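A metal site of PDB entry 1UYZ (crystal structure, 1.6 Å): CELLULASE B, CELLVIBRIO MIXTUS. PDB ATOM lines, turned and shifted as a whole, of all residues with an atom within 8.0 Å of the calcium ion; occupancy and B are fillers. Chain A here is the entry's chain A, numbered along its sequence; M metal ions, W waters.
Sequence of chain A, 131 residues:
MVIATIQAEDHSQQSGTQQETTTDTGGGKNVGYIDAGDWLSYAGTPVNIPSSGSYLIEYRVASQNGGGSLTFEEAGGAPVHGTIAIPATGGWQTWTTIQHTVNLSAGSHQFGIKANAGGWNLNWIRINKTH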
ATOM      1  N   ILE A   6      -0.012  26.341  24.931  1.00  0.00           N
ATOM      2  CA  ILE A   6      -1.381  26.701  24.548  1.00  0.00           C
ATOM      3  C   ILE A   6      -1.431  26.760  23.032  1.00  0.00           C
ATOM      4  O   ILE A   6      -0.735  27.562  22.416  1.00  0.00           O
ATOM      5  CB  ILE A   6      -1.758  28.071  25.143  1.00  0.00           C
ATOM      6  CG1 ILE A   6      -1.772  28.027  26.673  1.00  0.00           C
ATOM      7  CG2 ILE A   6      -3.134  28.526  24.622  1.00  0.00           C
ATOM      8  CD1 ILE A   6      -1.809  29.404  27.317  1.00  0.00           C
ATOM      9  N   GLN A   7      -2.229  25.907  22.412  1.00  0.00           N
ATOM     10  CA  GLN A   7      -2.474  26.001  20.968  1.00  0.00           C
ATOM     11  C   GLN A   7      -3.246  27.277  20.719  1.00  0.00           C
ATOM     12  O   GLN A   7      -4.191  27.580  21.436  1.00  0.00           O
ATOM     13  CB  GLN A   7      -3.226  24.780  20.461  1.00  0.00           C
ATOM     14  CG  GLN A   7      -2.372  23.506  20.554  1.00  0.00           C
ATOM     15  CD  GLN A   7      -1.163  23.569  19.653  1.00  0.00           C
ATOM     16  OE1 GLN A   7      -1.205  24.176  18.566  1.00  0.00           O
ATOM     17  NE2 GLN A   7      -0.051  22.958  20.100  1.00  0.00           N
ATOM     18  N   ALA A   8      -2.833  28.043  19.710  1.00  0.00           N
ATOM     19  CA  ALA A   8      -3.432  29.368  19.479  1.00  0.00           C
ATOM     20  C   ALA A   8      -4.926  29.294  19.206  1.00  0.00           C
ATOM     21  O   ALA A   8      -5.684  30.175  19.597  1.00  0.00           O
ATOM     22  CB  ALA A   8      -2.728  30.043  18.328  1.00  0.00           C
ATOM     23  N   GLU A   9      -5.337  28.221  18.540  1.00  0.00           N
ATOM     24  CA  GLU A   9      -6.713  27.963  18.178  1.00  0.00           C
ATOM     25  C   GLU A   9      -7.622  27.593  19.351  1.00  0.00           C
ATOM     26  O   GLU A   9      -8.844  27.596  19.202  1.00  0.00           O
ATOM     27  CB  GLU A   9      -6.776  26.866  17.099  1.00  0.00           C
ATOM     28  CG  GLU A   9      -6.242  25.491  17.513  1.00  0.00           C
ATOM     29  CD  GLU A   9      -4.763  25.278  17.241  1.00  0.00           C
ATOM     30  OE1 GLU A   9      -3.952  26.238  17.234  1.00  0.00           O
ATOM     31  OE2 GLU A   9      -4.363  24.092  17.052  1.00  0.00           O
ATOM     32  N   ASP A  10      -7.035  27.273  20.506  1.00  0.00           N
ATOM     33  CA  ASP A  10      -7.783  26.844  21.693  1.00  0.00           C
ATOM     34  C   ASP A  10      -8.158  28.018  22.603  1.00  0.00           C
ATOM     35  O   ASP A  10      -8.193  27.914  23.840  1.00  0.00           O
ATOM     36  CB  ASP A  10      -6.982  25.791  22.466  1.00  0.00           C
ATOM     37  CG  ASP A  10      -6.955  24.424  21.784  1.00  0.00           C
ATOM     38  OD1 ASP A  10      -7.744  24.183  20.825  1.00  0.00           O
ATOM     39  OD2 ASP A  10      -6.165  23.529  22.156  1.00  0.00           O
ATOM     40  N   GLU A  20      -7.200  28.075  10.465  1.00  0.00           N
ATOM     41  CA  GLU A  20      -6.875  27.381   9.226  1.00  0.00           C
ATOM     42  C   GLU A  20      -5.942  26.217   9.523  1.00  0.00           C
ATOM     43  O   GLU A  20      -5.330  26.147  10.580  1.00  0.00           O
ATOM     44  CB  GLU A  20      -6.287  28.331   8.183  1.00  0.00           C
ATOM     45  CG  GLU A  20      -4.943  28.948   8.535  1.00  0.00           C
ATOM     46  CD  GLU A  20      -4.619  30.252   7.792  1.00  0.00           C
ATOM     47  OE1 GLU A  20      -5.270  30.589   6.780  1.00  0.00           O
ATOM     48  OE2 GLU A  20      -3.681  30.956   8.230  1.00  0.00           O
ATOM     49  N   THR A  22      -2.646  24.107   9.470  1.00  0.00           N
ATOM     50  CA  THR A  22      -1.226  24.409   9.353  1.00  0.00           C
ATOM     51  C   THR A  22      -0.446  23.200   8.867  1.00  0.00           C
ATOM     52  O   THR A  22      -0.792  22.068   9.191  1.00  0.00           O
ATOM     53  CB  THR A  22      -0.643  24.926  10.693  1.00  0.00           C
ATOM     54  OG1 THR A  22       0.715  25.329  10.491  1.00  0.00           O
ATOM     55  CG2 THR A  22      -0.556  23.836  11.750  1.00  0.00           C
ATOM     56  N   ASP A  24       2.794  23.218   9.636  1.00  0.00           N
ATOM     57  CA  ASP A  24       3.902  23.206  10.580  1.00  0.00           C
ATOM     58  C   ASP A  24       4.037  21.821  11.217  1.00  0.00           C
ATOM     59  O   ASP A  24       3.107  21.033  11.183  1.00  0.00           O
ATOM     60  CB  ASP A  24       3.657  24.260  11.673  1.00  0.00           C
ATOM     61  CG  ASP A  24       4.895  24.547  12.495  1.00  0.00           C
ATOM     62  OD1 ASP A  24       6.042  24.264  12.039  1.00  0.00           O
ATOM     63  OD2 ASP A  24       4.809  25.077  13.621  1.00  0.00           O
ATOM     64  N   THR A  25       5.209  21.533  11.758  1.00  0.00           N
ATOM     65  CA  THR A  25       5.450  20.310  12.522  1.00  0.00           C
ATOM     66  C   THR A  25       4.339  20.047  13.538  1.00  0.00           C
ATOM     67  O   THR A  25       4.022  20.918  14.362  1.00  0.00           O
ATOM     68  CB  THR A  25       6.791  20.437  13.272  1.00  0.00           C
ATOM     69  OG1 THR A  25       7.807  20.907  12.385  1.00  0.00           O
ATOM     70  CG2 THR A  25       7.280  19.068  13.740  1.00  0.00           C
ATOM     71  N   GLY A  26       3.753  18.865  13.476  1.00  0.00           N
ATOM     72  CA  GLY A  26       2.703  18.463  14.396  1.00  0.00           C
ATOM     73  C   GLY A  26       1.304  18.660  13.833  1.00  0.00           C
ATOM     74  O   GLY A  26       0.327  18.195  14.429  1.00  0.00           O
ATOM     75  N   GLY A  27       1.209  19.354  12.711  1.00  0.00           N
ATOM     76  CA  GLY A  27      -0.065  19.625  12.058  1.00  0.00           C
ATOM     77  C   GLY A  27      -1.022  20.410  12.931  1.00  0.00           C
ATOM     78  O   GLY A  27      -0.621  21.256  13.733  1.00  0.00           O
ATOM     79  N   GLY A  28      -2.303  20.111  12.788  1.00  0.00           N
ATOM     80  CA  GLY A  28      -3.346  20.814  13.496  1.00  0.00           C
ATOM     81  C   GLY A  28      -3.726  22.105  12.805  1.00  0.00           C
ATOM     82  O   GLY A  28      -3.853  22.146  11.566  1.00  0.00           O
ATOM     83  N   LYS A  29      -3.900  23.160  13.605  1.00  0.00           N
ATOM     84  CA  LYS A  29      -4.410  24.425  13.114  1.00  0.00           C
ATOM     85  C   LYS A  29      -3.541  25.582  13.560  1.00  0.00           C
ATOM     86  O   LYS A  29      -2.804  25.465  14.540  1.00  0.00           O
ATOM     87  CB  LYS A  29      -5.836  24.645  13.631  1.00  0.00           C
ATOM     88  CG  LYS A  29      -6.811  23.567  13.208  1.00  0.00           C
ATOM     89  CD  LYS A  29      -8.173  23.732  13.834  1.00  0.00           C
ATOM     90  CE  LYS A  29      -9.144  22.662  13.320  1.00  0.00           C
ATOM     91  NZ  LYS A  29     -10.315  22.438  14.212  1.00  0.00           N
ATOM     92  N   ASN A  30      -3.598  26.677  12.809  1.00  0.00           N
ATOM     93  CA  ASN A  30      -3.098  27.957  13.280  1.00  0.00           C
ATOM     94  C   ASN A  30      -4.207  28.989  13.222  1.00  0.00           C
ATOM     95  O   ASN A  30      -5.218  28.805  12.552  1.00  0.00           O
ATOM     96  CB  ASN A  30      -1.855  28.429  12.491  1.00  0.00           C
ATOM     97  CG  ASN A  30      -2.165  28.840  11.054  1.00  0.00           C
ATOM     98  OD1 ASN A  30      -2.478  30.004  10.764  1.00  0.00           O
ATOM     99  ND2 ASN A  30      -2.042  27.899  10.132  1.00  0.00           N
ATOM    100  N   VAL A  31      -4.016  30.071  13.961  1.00  0.00           N
ATOM    101  CA  VAL A  31      -4.870  31.232  13.853  1.00  0.00           C
ATOM    102  C   VAL A  31      -4.277  32.111  12.767  1.00  0.00           C
ATOM    103  O   VAL A  31      -3.074  32.348  12.721  1.00  0.00           O
ATOM    104  CB  VAL A  31      -4.950  32.007  15.184  1.00  0.00           C
ATOM    105  CG1 VAL A  31      -5.760  33.297  15.002  1.00  0.00           C
ATOM    106  CG2 VAL A  31      -5.566  31.147  16.266  1.00  0.00           C
ATOM    107  N   ARG A  60       5.027  30.518  18.236  1.00  0.00           N
ATOM    108  CA  ARG A  60       5.289  29.842  16.970  1.00  0.00           C
ATOM    109  C   ARG A  60       4.540  30.601  15.882  1.00  0.00           C
ATOM    110  O   ARG A  60       3.308  30.572  15.827  1.00  0.00           O
ATOM    111  CB  ARG A  60       4.853  28.380  17.071  1.00  0.00           C
ATOM    112  CG  ARG A  60       5.245  27.510  15.892  1.00  0.00           C
ATOM    113  CD  ARG A  60       6.752  27.307  15.770  1.00  0.00           C
ATOM    114  NE  ARG A  60       7.067  26.358  14.722  1.00  0.00           N
ATOM    115  CZ  ARG A  60       8.293  26.079  14.300  1.00  0.00           C
ATOM    116  NH1 ARG A  60       9.335  26.655  14.865  1.00  0.00           N
ATOM    117  NH2 ARG A  60       8.478  25.212  13.318  1.00  0.00           N
ATOM    118  N   TRP A  95       7.471  28.529   9.353  1.00  0.00           N
ATOM    119  CA  TRP A  95       7.317  28.744  10.787  1.00  0.00           C
ATOM    120  C   TRP A  95       8.650  28.936  11.495  1.00  0.00           C
ATOM    121  O   TRP A  95       9.652  28.335  11.145  1.00  0.00           O
ATOM    122  CB  TRP A  95       6.555  27.562  11.385  1.00  0.00           C
ATOM    123  CG  TRP A  95       5.163  27.524  10.862  1.00  0.00           C
ATOM    124  CD1 TRP A  95       4.716  26.829   9.761  1.00  0.00           C
ATOM    125  CD2 TRP A  95       4.038  28.260  11.349  1.00  0.00           C
ATOM    126  NE1 TRP A  95       3.374  27.080   9.564  1.00  0.00           N
ATOM    127  CE2 TRP A  95       2.945  27.963  10.516  1.00  0.00           C
ATOM    128  CE3 TRP A  95       3.853  29.154  12.413  1.00  0.00           C
ATOM    129  CZ2 TRP A  95       1.676  28.513  10.731  1.00  0.00           C
ATOM    130  CZ3 TRP A  95       2.596  29.700  12.616  1.00  0.00           C
ATOM    131  CH2 TRP A  95       1.528  29.378  11.775  1.00  0.00           C
ATOM    132  N   LEU A 122      -0.282  32.441  13.918  1.00  0.00           N
ATOM    133  CA  LEU A 122       0.164  31.939  15.222  1.00  0.00           C
ATOM    134  C   LEU A 122      -0.280  30.499  15.383  1.00  0.00           C
ATOM    135  O   LEU A 122      -1.454  30.210  15.276  1.00  0.00           O
ATOM    136  CB  LEU A 122      -0.424  32.791  16.341  1.00  0.00           C
ATOM    137  CG  LEU A 122       0.031  32.486  17.771  1.00  0.00           C
ATOM    138  CD1 LEU A 122       1.485  32.824  17.960  1.00  0.00           C
ATOM    139  CD2 LEU A 122      -0.821  33.258  18.778  1.00  0.00           C
ATOM    140  N   ASN A 123       0.660  29.602  15.651  1.00  0.00           N
ATOM    141  CA  ASN A 123       0.335  28.176  15.808  1.00  0.00           C
ATOM    142  C   ASN A 123       0.073  27.826  17.278  1.00  0.00           C
ATOM    143  O   ASN A 123      -0.911  27.156  17.608  1.00  0.00           O
ATOM    144  CB  ASN A 123       1.475  27.332  15.233  1.00  0.00           C
ATOM    145  CG  ASN A 123       1.155  25.848  15.172  1.00  0.00           C
ATOM    146  OD1 ASN A 123       0.057  25.416  15.524  1.00  0.00           O
ATOM    147  ND2 ASN A 123       2.136  25.043  14.745  1.00  0.00           N
ATOM    148  N   TRP A 124       0.965  28.275  18.148  1.00  0.00           N
ATOM    149  CA  TRP A 124       0.904  28.009  19.575  1.00  0.00           C
ATOM    150  C   TRP A 124       1.803  28.985  20.341  1.00  0.00           C
ATOM    151  O   TRP A 124       2.612  29.713  19.755  1.00  0.00           O
ATOM    152  CB  TRP A 124       1.277  26.542  19.915  1.00  0.00           C
ATOM    153  CG  TRP A 124       2.561  25.994  19.302  1.00  0.00           C
ATOM    154  CD1 TRP A 124       2.649  25.135  18.237  1.00  0.00           C
ATOM    155  CD2 TRP A 124       3.916  26.230  19.719  1.00  0.00           C
ATOM    156  NE1 TRP A 124       3.969  24.836  17.967  1.00  0.00           N
ATOM    157  CE2 TRP A 124       4.770  25.505  18.865  1.00  0.00           C
ATOM    158  CE3 TRP A 124       4.498  26.998  20.741  1.00  0.00           C
ATOM    159  CZ2 TRP A 124       6.160  25.530  18.994  1.00  0.00           C
ATOM    160  CZ3 TRP A 124       5.869  27.023  20.859  1.00  0.00           C
ATOM    161  CH2 TRP A 124       6.695  26.286  19.990  1.00  0.00           C
ATOM    162  N   ILE A 125       1.611  28.996  21.656  1.00  0.00           N
ATOM    163  CA  ILE A 125       2.365  29.799  22.606  1.00  0.00           C
ATOM    164  C   ILE A 125       2.884  28.856  23.664  1.00  0.00           C
ATOM    165  O   ILE A 125       2.229  27.867  23.989  1.00  0.00           O
ATOM    166  CB  ILE A 125       1.430  30.834  23.276  1.00  0.00           C
ATOM    167  CG1 ILE A 125       0.668  31.655  22.218  1.00  0.00           C
ATOM    168  CG2 ILE A 125       2.197  31.732  24.237  1.00  0.00           C
ATOM    169  CD1 ILE A 125      -0.849  31.549  22.366  1.00  0.00           C
HETATM  170 CA    CA M   1      -1.929  25.062  16.627  1.00  0.00          CA
HETATM  171  O   HOH W   1      -1.857  22.779  15.965  1.00  0.00           O
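N of Ala 8 lies close to O of Asn 123 (3.0 Å). The side-chain amide nitrogen of Asn 123 lies within hydrogen-bond range of the side-chain carboxylate of Asp 24. The backbone NH (N) of Asn 123 lies within hydrogen-bond range of the backbone carbonyl oxygen (O) of Arg 60 (2.8 Å).
The calcium ion is bound by OE1 of Gln 7 (2.3 Å), O of Lys 29 (2.3 Å), OD1 of Asn 123 (2.3 Å), water W1 (2.4 Å), OE1 of Glu 9 (2.4 Å), O of Asn 123 (2.5 Å) and OE2 of Glu 9 (2.7 Å). The calcium ion has seven donor atoms within binding distance.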
